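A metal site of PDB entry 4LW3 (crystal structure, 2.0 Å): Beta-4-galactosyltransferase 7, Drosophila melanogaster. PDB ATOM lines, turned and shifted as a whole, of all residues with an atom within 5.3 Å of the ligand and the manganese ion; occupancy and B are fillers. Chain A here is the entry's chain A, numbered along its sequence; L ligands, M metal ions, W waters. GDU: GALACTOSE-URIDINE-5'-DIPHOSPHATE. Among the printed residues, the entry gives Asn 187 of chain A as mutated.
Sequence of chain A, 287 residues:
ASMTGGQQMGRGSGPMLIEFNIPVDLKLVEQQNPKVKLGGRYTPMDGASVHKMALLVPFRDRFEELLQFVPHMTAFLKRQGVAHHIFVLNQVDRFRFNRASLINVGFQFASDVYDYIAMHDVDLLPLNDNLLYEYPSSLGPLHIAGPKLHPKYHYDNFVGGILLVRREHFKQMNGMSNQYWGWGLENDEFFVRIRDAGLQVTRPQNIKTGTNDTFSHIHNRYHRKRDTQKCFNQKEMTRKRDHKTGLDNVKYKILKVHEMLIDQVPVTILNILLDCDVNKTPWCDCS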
ATOM      1  N   VAL A  57       5.170   6.632  29.348  1.00  0.00           N
ATOM      2  CA  VAL A  57       6.114   7.368  28.520  1.00  0.00           C
ATOM      3  C   VAL A  57       7.523   6.802  28.684  1.00  0.00           C
ATOM      4  O   VAL A  57       8.244   7.202  29.608  1.00  0.00           O
ATOM      5  CB  VAL A  57       6.173   8.856  28.910  1.00  0.00           C
ATOM      6  CG1 VAL A  57       7.044   9.633  27.914  1.00  0.00           C
ATOM      7  CG2 VAL A  57       4.769   9.460  28.962  1.00  0.00           C
ATOM      8  N   PRO A  58       7.895   5.857  27.811  1.00  0.00           N
ATOM      9  CA  PRO A  58       9.280   5.355  27.783  1.00  0.00           C
ATOM     10  C   PRO A  58      10.205   6.525  27.590  1.00  0.00           C
ATOM     11  O   PRO A  58       9.906   7.435  26.805  1.00  0.00           O
ATOM     12  CB  PRO A  58       9.308   4.423  26.559  1.00  0.00           C
ATOM     13  CG  PRO A  58       7.967   4.596  25.848  1.00  0.00           C
ATOM     14  CD  PRO A  58       7.012   5.163  26.854  1.00  0.00           C
ATOM     15  N   PHE A  59      11.314   6.542  28.320  1.00  0.00           N
ATOM     16  CA  PHE A  59      12.063   7.778  28.446  1.00  0.00           C
ATOM     17  C   PHE A  59      13.532   7.535  28.746  1.00  0.00           C
ATOM     18  O   PHE A  59      13.878   6.680  29.562  1.00  0.00           O
ATOM     19  CB  PHE A  59      11.440   8.578  29.587  1.00  0.00           C
ATOM     20  CG  PHE A  59      12.066   9.927  29.818  1.00  0.00           C
ATOM     21  CD1 PHE A  59      13.201  10.063  30.608  1.00  0.00           C
ATOM     22  CD2 PHE A  59      11.495  11.065  29.259  1.00  0.00           C
ATOM     23  CE1 PHE A  59      13.782  11.306  30.816  1.00  0.00           C
ATOM     24  CE2 PHE A  59      12.063  12.313  29.463  1.00  0.00           C
ATOM     25  CZ  PHE A  59      13.203  12.441  30.251  1.00  0.00           C
ATOM     26  N   ARG A  60      14.378   8.285  28.041  1.00  0.00           N
ATOM     27  CA  ARG A  60      15.783   8.448  28.425  1.00  0.00           C
ATOM     28  C   ARG A  60      16.330   9.685  27.742  1.00  0.00           C
ATOM     29  O   ARG A  60      16.226   9.840  26.516  1.00  0.00           O
ATOM     30  CB  ARG A  60      16.622   7.229  28.065  1.00  0.00           C
ATOM     31  CG  ARG A  60      18.125   7.455  28.270  1.00  0.00           C
ATOM     32  CD  ARG A  60      18.933   6.464  27.468  1.00  0.00           C
ATOM     33  NE  ARG A  60      19.116   5.227  28.226  1.00  0.00           N
ATOM     34  CZ  ARG A  60      19.557   4.090  27.707  1.00  0.00           C
ATOM     35  NH1 ARG A  60      19.838   3.993  26.414  1.00  0.00           N
ATOM     36  NH2 ARG A  60      19.697   3.034  28.500  1.00  0.00           N
ATOM     37  N   ASP A  61      16.899  10.583  28.542  1.00  0.00           N
ATOM     38  CA  ASP A  61      17.555  11.789  28.026  1.00  0.00           C
ATOM     39  C   ASP A  61      16.634  12.679  27.172  1.00  0.00           C
ATOM     40  O   ASP A  61      17.044  13.155  26.125  1.00  0.00           O
ATOM     41  CB  ASP A  61      18.773  11.399  27.173  1.00  0.00           C
ATOM     42  CG  ASP A  61      19.854  10.669  27.975  1.00  0.00           C
ATOM     43  OD1 ASP A  61      19.912  10.820  29.209  1.00  0.00           O
ATOM     44  OD2 ASP A  61      20.645   9.932  27.344  1.00  0.00           O
ATOM     45  N   ARG A  62      15.396  12.905  27.634  1.00  0.00           N
ATOM     46  CA  ARG A  62      14.470  13.769  26.904  1.00  0.00           C
ATOM     47  C   ARG A  62      13.783  14.744  27.848  1.00  0.00           C
ATOM     48  O   ARG A  62      12.591  14.993  27.734  1.00  0.00           O
ATOM     49  CB  ARG A  62      13.411  12.943  26.160  1.00  0.00           C
ATOM     50  CG  ARG A  62      13.971  11.960  25.144  1.00  0.00           C
ATOM     51  CD  ARG A  62      14.643  12.692  23.966  1.00  0.00           C
ATOM     52  NE  ARG A  62      15.116  11.751  22.956  1.00  0.00           N
ATOM     53  CZ  ARG A  62      16.357  11.272  22.881  1.00  0.00           C
ATOM     54  NH1 ARG A  62      17.265  11.664  23.770  1.00  0.00           N
ATOM     55  NH2 ARG A  62      16.695  10.424  21.933  1.00  0.00           N
ATOM     56  N   PHE A  97      18.421   1.879  24.030  1.00  0.00           N
ATOM     57  CA  PHE A  97      17.062   2.206  24.426  1.00  0.00           C
ATOM     58  C   PHE A  97      16.054   1.121  24.026  1.00  0.00           C
ATOM     59  O   PHE A  97      15.967   0.768  22.847  1.00  0.00           O
ATOM     60  CB  PHE A  97      16.650   3.548  23.829  1.00  0.00           C
ATOM     61  CG  PHE A  97      15.373   4.082  24.392  1.00  0.00           C
ATOM     62  CD1 PHE A  97      15.303   4.491  25.715  1.00  0.00           C
ATOM     63  CD2 PHE A  97      14.234   4.160  23.601  1.00  0.00           C
ATOM     64  CE1 PHE A  97      14.118   4.981  26.248  1.00  0.00           C
ATOM     65  CE2 PHE A  97      13.037   4.642  24.137  1.00  0.00           C
ATOM     66  CZ  PHE A  97      12.980   5.046  25.463  1.00  0.00           C
ATOM     67  N   ARG A  99      12.240   0.710  24.332  1.00  0.00           N
ATOM     68  CA  ARG A  99      10.980   1.308  24.788  1.00  0.00           C
ATOM     69  C   ARG A  99       9.929   0.251  25.125  1.00  0.00           C
ATOM     70  O   ARG A  99       9.126   0.442  26.036  1.00  0.00           O
ATOM     71  CB  ARG A  99      10.444   2.334  23.771  1.00  0.00           C
ATOM     72  CG  ARG A  99       9.832   1.757  22.516  1.00  0.00           C
ATOM     73  CD  ARG A  99       9.333   2.879  21.576  1.00  0.00           C
ATOM     74  NE  ARG A  99       8.131   3.547  22.040  1.00  0.00           N
ATOM     75  CZ  ARG A  99       6.897   3.070  21.851  1.00  0.00           C
ATOM     76  NH1 ARG A  99       6.717   1.913  21.226  1.00  0.00           N
ATOM     77  NH2 ARG A  99       5.837   3.723  22.292  1.00  0.00           N
ATOM     78  N   HIS A 120       2.967   6.179  24.753  1.00  0.00           N
ATOM     79  CA  HIS A 120       3.024   7.530  24.191  1.00  0.00           C
ATOM     80  C   HIS A 120       4.459   8.036  24.030  1.00  0.00           C
ATOM     81  O   HIS A 120       5.203   8.075  25.004  1.00  0.00           O
ATOM     82  CB  HIS A 120       2.288   8.457  25.157  1.00  0.00           C
ATOM     83  CG  HIS A 120       1.570   9.595  24.496  1.00  0.00           C
ATOM     84  ND1 HIS A 120       2.210  10.575  23.771  1.00  0.00           N
ATOM     85  CD2 HIS A 120       0.249   9.927  24.492  1.00  0.00           C
ATOM     86  CE1 HIS A 120       1.320  11.449  23.334  1.00  0.00           C
ATOM     87  NE2 HIS A 120       0.126  11.076  23.752  1.00  0.00           N
ATOM     88  N   ASP A 121       4.855   8.421  22.806  1.00  0.00           N
ATOM     89  CA  ASP A 121       6.141   9.090  22.601  1.00  0.00           C
ATOM     90  C   ASP A 121       6.112  10.445  23.313  1.00  0.00           C
ATOM     91  O   ASP A 121       5.066  11.100  23.353  1.00  0.00           O
ATOM     92  CB  ASP A 121       6.421   9.322  21.122  1.00  0.00           C
ATOM     93  CG  ASP A 121       6.550   8.039  20.327  1.00  0.00           C
ATOM     94  OD1 ASP A 121       6.555   6.948  20.951  1.00  0.00           O
ATOM     95  OD2 ASP A 121       6.647   8.117  19.082  1.00  0.00           O
ATOM     96  N   VAL A 122       7.250  10.874  23.845  1.00  0.00           N
ATOM     97  CA  VAL A 122       7.283  12.102  24.628  1.00  0.00           C
ATOM     98  C   VAL A 122       7.298  13.352  23.739  1.00  0.00           C
ATOM     99  O   VAL A 122       7.034  14.466  24.209  1.00  0.00           O
ATOM    100  CB  VAL A 122       8.503  12.112  25.578  1.00  0.00           C
ATOM    101  CG1 VAL A 122       9.772  12.430  24.795  1.00  0.00           C
ATOM    102  CG2 VAL A 122       8.300  13.106  26.723  1.00  0.00           C
ATOM    103  N   ASP A 123       7.582  13.172  22.449  1.00  0.00           N
ATOM    104  CA  ASP A 123       7.791  14.304  21.539  1.00  0.00           C
ATOM    105  C   ASP A 123       6.611  14.515  20.577  1.00  0.00           C
ATOM    106  O   ASP A 123       6.703  15.303  19.616  1.00  0.00           O
ATOM    107  CB  ASP A 123       9.054  14.069  20.701  1.00  0.00           C
ATOM    108  CG  ASP A 123       8.957  12.806  19.865  1.00  0.00           C
ATOM    109  OD1 ASP A 123       7.880  12.160  19.885  1.00  0.00           O
ATOM    110  OD2 ASP A 123       9.945  12.445  19.178  1.00  0.00           O
ATOM    111  N   LEU A 124       5.520  13.808  20.822  1.00  0.00           N
ATOM    112  CA  LEU A 124       4.412  13.783  19.870  1.00  0.00           C
ATOM    113  C   LEU A 124       3.136  14.289  20.532  1.00  0.00           C
ATOM    114  O   LEU A 124       2.546  13.587  21.361  1.00  0.00           O
ATOM    115  CB  LEU A 124       4.220  12.353  19.331  1.00  0.00           C
ATOM    116  CG  LEU A 124       3.211  12.178  18.187  1.00  0.00           C
ATOM    117  CD1 LEU A 124       3.671  12.961  16.968  1.00  0.00           C
ATOM    118  CD2 LEU A 124       3.047  10.695  17.847  1.00  0.00           C
ATOM    119  N   HIS A 150      -0.320  11.116  11.061  1.00  0.00           N
ATOM    120  CA  HIS A 150       1.035  11.266  11.553  1.00  0.00           C
ATOM    121  C   HIS A 150       1.891  12.037  10.545  1.00  0.00           C
ATOM    122  O   HIS A 150       1.767  11.837   9.337  1.00  0.00           O
ATOM    123  CB  HIS A 150       1.658   9.905  11.864  1.00  0.00           C
ATOM    124  CG  HIS A 150       2.910   9.992  12.697  1.00  0.00           C
ATOM    125  ND1 HIS A 150       4.143  10.289  12.164  1.00  0.00           N
ATOM    126  CD2 HIS A 150       3.103   9.834  14.033  1.00  0.00           C
ATOM    127  CE1 HIS A 150       5.045  10.319  13.126  1.00  0.00           C
ATOM    128  NE2 HIS A 150       4.441  10.047  14.272  1.00  0.00           N
ATOM    129  N   TYR A 153       5.090   8.970   9.525  1.00  0.00           N
ATOM    130  CA  TYR A 153       4.888   7.559   9.234  1.00  0.00           C
ATOM    131  C   TYR A 153       3.499   7.343   8.647  1.00  0.00           C
ATOM    132  O   TYR A 153       2.489   7.671   9.276  1.00  0.00           O
ATOM    133  CB  TYR A 153       5.121   6.692  10.483  1.00  0.00           C
ATOM    134  CG  TYR A 153       6.538   6.823  11.007  1.00  0.00           C
ATOM    135  CD1 TYR A 153       7.612   6.288  10.313  1.00  0.00           C
ATOM    136  CD2 TYR A 153       6.806   7.500  12.195  1.00  0.00           C
ATOM    137  CE1 TYR A 153       8.910   6.406  10.793  1.00  0.00           C
ATOM    138  CE2 TYR A 153       8.086   7.632  12.674  1.00  0.00           C
ATOM    139  CZ  TYR A 153       9.146   7.079  11.974  1.00  0.00           C
ATOM    140  OH  TYR A 153      10.430   7.216  12.445  1.00  0.00           O
ATOM    141  N   PHE A 158       1.134   1.034  10.506  1.00  0.00           N
ATOM    142  CA  PHE A 158       1.813   1.813  11.534  1.00  0.00           C
ATOM    143  C   PHE A 158       0.903   1.962  12.747  1.00  0.00           C
ATOM    144  O   PHE A 158      -0.235   2.414  12.630  1.00  0.00           O
ATOM    145  CB  PHE A 158       2.145   3.206  10.986  1.00  0.00           C
ATOM    146  CG  PHE A 158       2.722   4.139  12.016  1.00  0.00           C
ATOM    147  CD1 PHE A 158       4.028   3.967  12.479  1.00  0.00           C
ATOM    148  CD2 PHE A 158       1.978   5.197  12.507  1.00  0.00           C
ATOM    149  CE1 PHE A 158       4.574   4.847  13.421  1.00  0.00           C
ATOM    150  CE2 PHE A 158       2.503   6.086  13.457  1.00  0.00           C
ATOM    151  CZ  PHE A 158       3.814   5.905  13.917  1.00  0.00           C
ATOM    152  N   GLY A 160       2.423   3.206  15.824  1.00  0.00           N
ATOM    153  CA  GLY A 160       3.327   3.817  16.779  1.00  0.00           C
ATOM    154  C   GLY A 160       2.899   5.187  17.266  1.00  0.00           C
ATOM    155  O   GLY A 160       1.779   5.635  16.989  1.00  0.00           O
ATOM    156  N   GLY A 161       3.788   5.865  17.998  1.00  0.00           N
ATOM    157  CA  GLY A 161       3.495   7.204  18.460  1.00  0.00           C
ATOM    158  C   GLY A 161       2.582   7.255  19.676  1.00  0.00           C
ATOM    159  O   GLY A 161       3.025   7.580  20.781  1.00  0.00           O
ATOM    160  N   GLY A 182      17.378  -0.487  20.794  1.00  0.00           N
ATOM    161  CA  GLY A 182      17.658   0.487  19.750  1.00  0.00           C
ATOM    162  C   GLY A 182      16.372   0.764  18.964  1.00  0.00           C
ATOM    163  O   GLY A 182      15.354   0.121  19.183  1.00  0.00           O
ATOM    164  N   TRP A 183      16.446   1.722  18.044  1.00  0.00           N
ATOM    165  CA  TRP A 183      15.257   2.164  17.306  1.00  0.00           C
ATOM    166  C   TRP A 183      14.619   1.077  16.434  1.00  0.00           C
ATOM    167  O   TRP A 183      15.315   0.235  15.843  1.00  0.00           O
ATOM    168  CB  TRP A 183      15.617   3.370  16.418  1.00  0.00           C
ATOM    169  CG  TRP A 183      14.423   3.928  15.644  1.00  0.00           C
ATOM    170  CD1 TRP A 183      13.594   4.954  16.021  1.00  0.00           C
ATOM    171  CD2 TRP A 183      13.941   3.472  14.364  1.00  0.00           C
ATOM    172  NE1 TRP A 183      12.628   5.164  15.055  1.00  0.00           N
ATOM    173  CE2 TRP A 183      12.823   4.264  14.027  1.00  0.00           C
ATOM    174  CE3 TRP A 183      14.354   2.485  13.474  1.00  0.00           C
ATOM    175  CZ2 TRP A 183      12.112   4.091  12.835  1.00  0.00           C
ATOM    176  CZ3 TRP A 183      13.652   2.302  12.293  1.00  0.00           C
ATOM    177  CH2 TRP A 183      12.537   3.098  11.986  1.00  0.00           C
ATOM    178  N   GLY A 184      13.285   1.103  16.379  1.00  0.00           N
ATOM    179  CA  GLY A 184      12.527   0.439  15.328  1.00  0.00           C
ATOM    180  C   GLY A 184      11.878  -0.892  15.620  1.00  0.00           C
ATOM    181  O   GLY A 184      12.273  -1.594  16.554  1.00  0.00           O
ATOM    182  N   LEU A 185      10.865  -1.216  14.819  1.00  0.00           N
ATOM    183  CA  LEU A 185      10.246  -2.545  14.706  1.00  0.00           C
ATOM    184  C   LEU A 185       9.364  -3.039  15.866  1.00  0.00           C
ATOM    185  O   LEU A 185       8.505  -3.909  15.661  1.00  0.00           O
ATOM    186  CB  LEU A 185      11.308  -3.607  14.352  1.00  0.00           C
ATOM    187  CG  LEU A 185      11.934  -3.515  12.957  1.00  0.00           C
ATOM    188  CD1 LEU A 185      12.981  -4.605  12.758  1.00  0.00           C
ATOM    189  CD2 LEU A 185      10.855  -3.606  11.878  1.00  0.00           C
ATOM    190  N   GLU A 186       9.572  -2.511  17.072  1.00  0.00           N
ATOM    191  CA  GLU A 186       8.864  -3.065  18.224  1.00  0.00           C
ATOM    192  C   GLU A 186       7.343  -2.910  18.124  1.00  0.00           C
ATOM    193  O   GLU A 186       6.595  -3.789  18.559  1.00  0.00           O
ATOM    194  CB  GLU A 186       9.399  -2.495  19.549  1.00  0.00           C
ATOM    195  CG  GLU A 186       8.737  -1.215  20.026  1.00  0.00           C
ATOM    196  CD  GLU A 186       9.080  -0.014  19.164  1.00  0.00           C
ATOM    197  OE1 GLU A 186      10.161  -0.008  18.530  1.00  0.00           O
ATOM    198  OE2 GLU A 186       8.272   0.937  19.135  1.00  0.00           O
ATOM    199  N   ASN A 187       6.883  -1.806  17.539  1.00  0.00           N
ATOM    200  CA  ASN A 187       5.437  -1.581  17.392  1.00  0.00           C
ATOM    201  C   ASN A 187       4.872  -2.417  16.261  1.00  0.00           C
ATOM    202  O   ASN A 187       3.696  -2.797  16.275  1.00  0.00           O
ATOM    203  CB  ASN A 187       5.135  -0.099  17.168  1.00  0.00           C
ATOM    204  CG  ASN A 187       4.826   0.636  18.447  1.00  0.00           C
ATOM    205  OD1 ASN A 187       4.176   0.095  19.342  1.00  0.00           O
ATOM    206  ND2 ASN A 187       5.279   1.890  18.557  1.00  0.00           N
ATOM    207  N   HIS A 217       5.271  17.012  15.997  1.00  0.00           N
ATOM    208  CA  HIS A 217       6.348  16.058  16.228  1.00  0.00           C
ATOM    209  C   HIS A 217       7.645  16.830  16.232  1.00  0.00           C
ATOM    210  O   HIS A 217       8.272  17.015  15.187  1.00  0.00           O
ATOM    211  CB  HIS A 217       6.394  14.990  15.136  1.00  0.00           C
ATOM    212  CG  HIS A 217       7.424  13.917  15.385  1.00  0.00           C
ATOM    213  ND1 HIS A 217       8.069  13.256  14.352  1.00  0.00           N
ATOM    214  CD2 HIS A 217       7.905  13.387  16.532  1.00  0.00           C
ATOM    215  CE1 HIS A 217       8.899  12.361  14.860  1.00  0.00           C
ATOM    216  NE2 HIS A 217       8.821  12.417  16.183  1.00  0.00           N
ATOM    217  N   HIS A 219      11.035  16.681  16.774  1.00  0.00           N
ATOM    218  CA  HIS A 219      12.077  15.681  16.882  1.00  0.00           C
ATOM    219  C   HIS A 219      13.005  15.931  15.701  1.00  0.00           C
ATOM    220  O   HIS A 219      12.723  15.527  14.581  1.00  0.00           O
ATOM    221  CB  HIS A 219      11.474  14.270  16.792  1.00  0.00           C
ATOM    222  CG  HIS A 219      12.479  13.161  16.866  1.00  0.00           C
ATOM    223  ND1 HIS A 219      12.111  11.829  16.997  1.00  0.00           N
ATOM    224  CD2 HIS A 219      13.832  13.173  16.825  1.00  0.00           C
ATOM    225  CE1 HIS A 219      13.203  11.085  17.029  1.00  0.00           C
ATOM    226  NE2 HIS A 219      14.258  11.873  16.930  1.00  0.00           N
ATOM    227  N   LYS A 225      19.142  11.616  17.982  1.00  0.00           N
ATOM    228  CA  LYS A 225      19.420  10.626  16.943  1.00  0.00           C
ATOM    229  C   LYS A 225      18.641   9.333  17.163  1.00  0.00           C
ATOM    230  O   LYS A 225      18.395   8.931  18.302  1.00  0.00           O
ATOM    231  CB  LYS A 225      20.914  10.305  16.851  1.00  0.00           C
ATOM    232  CG  LYS A 225      21.712  11.388  16.143  1.00  0.00           C
ATOM    233  CD  LYS A 225      23.182  11.021  16.037  1.00  0.00           C
ATOM    234  CE  LYS A 225      23.979  12.104  15.328  1.00  0.00           C
ATOM    235  NZ  LYS A 225      23.784  13.443  15.956  1.00  0.00           N
ATOM    236  N   ARG A 226      18.230   8.713  16.064  1.00  0.00           N
ATOM    237  CA  ARG A 226      17.639   7.388  16.121  1.00  0.00           C
ATOM    238  C   ARG A 226      18.764   6.361  16.116  1.00  0.00           C
ATOM    239  O   ARG A 226      19.642   6.394  15.251  1.00  0.00           O
ATOM    240  CB  ARG A 226      16.685   7.171  14.942  1.00  0.00           C
ATOM    241  CG  ARG A 226      15.447   8.069  14.990  1.00  0.00           C
ATOM    242  CD  ARG A 226      14.518   7.867  13.770  1.00  0.00           C
ATOM    243  NE  ARG A 226      13.285   8.615  13.973  1.00  0.00           N
ATOM    244  CZ  ARG A 226      13.129   9.907  13.672  1.00  0.00           C
ATOM    245  NH1 ARG A 226      14.140  10.591  13.129  1.00  0.00           N
ATOM    246  NH2 ARG A 226      11.973  10.522  13.912  1.00  0.00           N
HETATM  247  N1  GDU L   1      12.850   7.837  23.470  1.00  0.00           N
HETATM  248  C2  GDU L   1      13.610   8.295  24.487  1.00  0.00           C
HETATM  249  N3  GDU L   1      14.924   8.242  24.425  1.00  0.00           N
HETATM  250  C4  GDU L   1      15.558   7.717  23.353  1.00  0.00           C
HETATM  251  C5  GDU L   1      14.804   7.209  22.270  1.00  0.00           C
HETATM  252  C6  GDU L   1      13.393   7.301  22.369  1.00  0.00           C
HETATM  253  O2  GDU L   1      13.084   8.770  25.458  1.00  0.00           O
HETATM  254  O4  GDU L   1      16.967   7.656  23.310  1.00  0.00           O
HETATM  255  C1D GDU L   1      11.466   7.875  23.563  1.00  0.00           C
HETATM  256  C2D GDU L   1      10.823   9.243  23.309  1.00  0.00           C
HETATM  257  O2D GDU L   1       9.656   9.327  24.080  1.00  0.00           O
HETATM  258  C3D GDU L   1      10.511   9.165  21.871  1.00  0.00           C
HETATM  259  C4D GDU L   1      10.010   7.761  21.762  1.00  0.00           C
HETATM  260  O4D GDU L   1      10.895   6.962  22.600  1.00  0.00           O
HETATM  261  O3D GDU L   1       9.535  10.112  21.459  1.00  0.00           O
HETATM  262  C5D GDU L   1      10.031   7.243  20.335  1.00  0.00           C
HETATM  263  O5D GDU L   1      11.369   7.213  19.865  1.00  0.00           O
HETATM  264  PA  GDU L   1      11.797   8.191  18.657  1.00  0.00           P
HETATM  265  O1A GDU L   1      11.073   9.535  18.820  1.00  0.00           O
HETATM  266  O2A GDU L   1      13.288   8.351  18.688  1.00  0.00           O
HETATM  267  O3A GDU L   1      11.435   7.495  17.256  1.00  0.00           O
HETATM  268  PB  GDU L   1      10.333   7.870  16.177  1.00  0.00           P
HETATM  269  O1B GDU L   1      10.206   9.400  16.112  1.00  0.00           O
HETATM  270  O2B GDU L   1      10.798   7.277  14.861  1.00  0.00           O
HETATM  271  O3B GDU L   1       8.938   7.235  16.665  1.00  0.00           O
HETATM  272  C1' GDU L   1       8.355   6.069  16.055  1.00  0.00           C
HETATM  273  C2' GDU L   1       7.211   5.662  16.824  1.00  0.00           C
HETATM  274  C3' GDU L   1       7.605   5.215  18.129  1.00  0.00           C
HETATM  275  C4' GDU L   1       8.463   4.007  18.067  1.00  0.00           C
HETATM  276  C5' GDU L   1       9.790   4.203  17.202  1.00  0.00           C
HETATM  277  C6' GDU L   1      10.320   2.968  16.876  1.00  0.00           C
HETATM  278  O2' GDU L   1       6.283   6.866  16.962  1.00  0.00           O
HETATM  279  O3' GDU L   1       6.370   4.926  18.921  1.00  0.00           O
HETATM  280  O4' GDU L   1       7.719   2.927  17.488  1.00  0.00           O
HETATM  281  O5' GDU L   1       9.371   5.010  15.935  1.00  0.00           O
HETATM  282  O6' GDU L   1      11.098   2.543  17.819  1.00  0.00           O
HETATM  283 MN    MN M   1      10.082  11.020  17.509  1.00  0.00          MN
HETATM  284  O   HOH W   1       8.059   3.908  13.601  1.00  0.00           O
HETATM  285  O   HOH W   2       8.142   7.657  24.944  1.00  0.00           O
HETATM  286  O   HOH W   3       8.039  10.257  18.208  1.00  0.00           O
HETATM  287  O   HOH W   4       6.515   2.266  14.978  1.00  0.00           O
HETATM  288  O   HOH W   5      18.235   5.972  21.615  1.00  0.00           O
HETATM  289  O   HOH W   6      13.489  10.749  20.954  1.00  0.00           O
HETATM  290  O   HOH W   7      14.234   5.697  19.323  1.00  0.00           O
HETATM  291  O   HOH W   8      15.698   9.517  19.293  1.00  0.00           O
HETATM  292  O   HOH W   9       6.574   9.451  15.820  1.00  0.00           O
HETATM  293  O   HOH W  10      12.573   3.681  20.246  1.00  0.00           O
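CA of Phe 59 touches O2 of the ligand, 3.3 Å away.
Phe 97 touches the ligand.
Arg 99 touches the ligand.
Gly 160 touches the ligand.
Of the 28 residues printed, 19 come within 4 Å of the ligand.
The nearest printed residue that does not touch the ligand is Phe 158 (4.04 Å).
N of Gly 182 is in hydrogen-bond range of O of Phe 97, 2.8 Å away.
The backbone carbonyl oxygen (O) of Gly 161 lies within hydrogen-bond range of the backbone NH (N) of Asp 121.
ND1 of His 150 is in hydrogen-bond range of N of Tyr 153.
The side-chain amide nitrogen (ND2) of Asn 187 sits close to the guanidinium group (NH1) of Arg 99, 3.0 Å away.
ND1 of His 219 sits close to NH2 of Arg 226.
O of Arg 60 lies close to NH1 of Arg 62 (3.5 Å).
OD1 of Asp 121 lies within salt-bridge range of NH2 of Arg 99.
The guanidinium group (NH1) of Arg 99 lies within salt-bridge range of the side-chain carboxylate (OE2) of Glu 186 (2.8 Å).
The side-chain hydroxyl (OH) of Tyr 153 lies within hydrogen-bond range of an oxygen (O2B) of the ligand, 2.4 Å away.
The guanidinium group (NE) of Arg 226 is in salt-bridge range of an oxygen (O2B) of the ligand, at 3.0 Å.
N of Arg 60 sits at hydrogen-bond distance from O2 of the ligand.
The indole nitrogen of Trp 183 lies within hydrogen-bond range of an oxygen (O2B) of the ligand.
NH2 of Arg 62 sits at hydrogen-bond distance from O4 of the ligand, at 3.1 Å.
The backbone NH (N) of Gly 184 lies within hydrogen-bond range of an oxygen (O6') of the ligand.
O of Arg 60 is in hydrogen-bond range of N3 of the ligand (2.9 Å).
OD2 of Asp 121 is in hydrogen-bond range of O2' of the ligand.
The backbone NH of Val 122 lies within hydrogen-bond range of an oxygen (O2D) of the ligand, at 2.9 Å.
O4' of the ligand sits at hydrogen-bond distance from OE2 of Glu 186 (2.6 Å).
The backbone carbonyl oxygen of Pro 58 sits at hydrogen-bond distance from an oxygen (O2D) of the ligand.
ND2 of Asn 187 sits at hydrogen-bond distance from O4' of the ligand (2.9 Å).
O2' of the ligand is in hydrogen-bond range of N of Gly 161 (2.9 Å).
The manganese ion is bound by an oxygen (O1B) of the ligand (2.1 Å), the side-chain carboxylate of Asp 123 (2.2 Å), an oxygen (O1A) of the ligand (2.2 Å), a ring nitrogen (ND1) of His 219 (2.2 Å), water W3 (2.3 Å) and a ring nitrogen (NE2) of His 217 (2.3 Å).
The manganese ion has six donor atoms within binding distance.
Of the 28 residues printed, 3 come within 4 Å of the manganese ion.
Water W3 bridges the side-chain carboxylate (OD1) of Asp 123 (2.5 Å) and the side-chain carboxylate (OD2) of Asp 121 (2.7 Å).
Water W2 lies within hydrogen-bond range of O2D of the ligand, O of Pro 58 and O of His 120.
Water W8 lies within hydrogen-bond range of O2A of the ligand (2.7 Å), O of Lys 225 (2.9 Å) and NH2 of Arg 62 (3.0 Å).
Water W9 bridges a ring nitrogen (NE2) of His 150 (2.7 Å) and an oxygen (O2') of the ligand (2.8 Å).
Water W6 lies within hydrogen-bond range of NE of Arg 62 (2.8 Å) and O2A of the ligand (3.3 Å).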
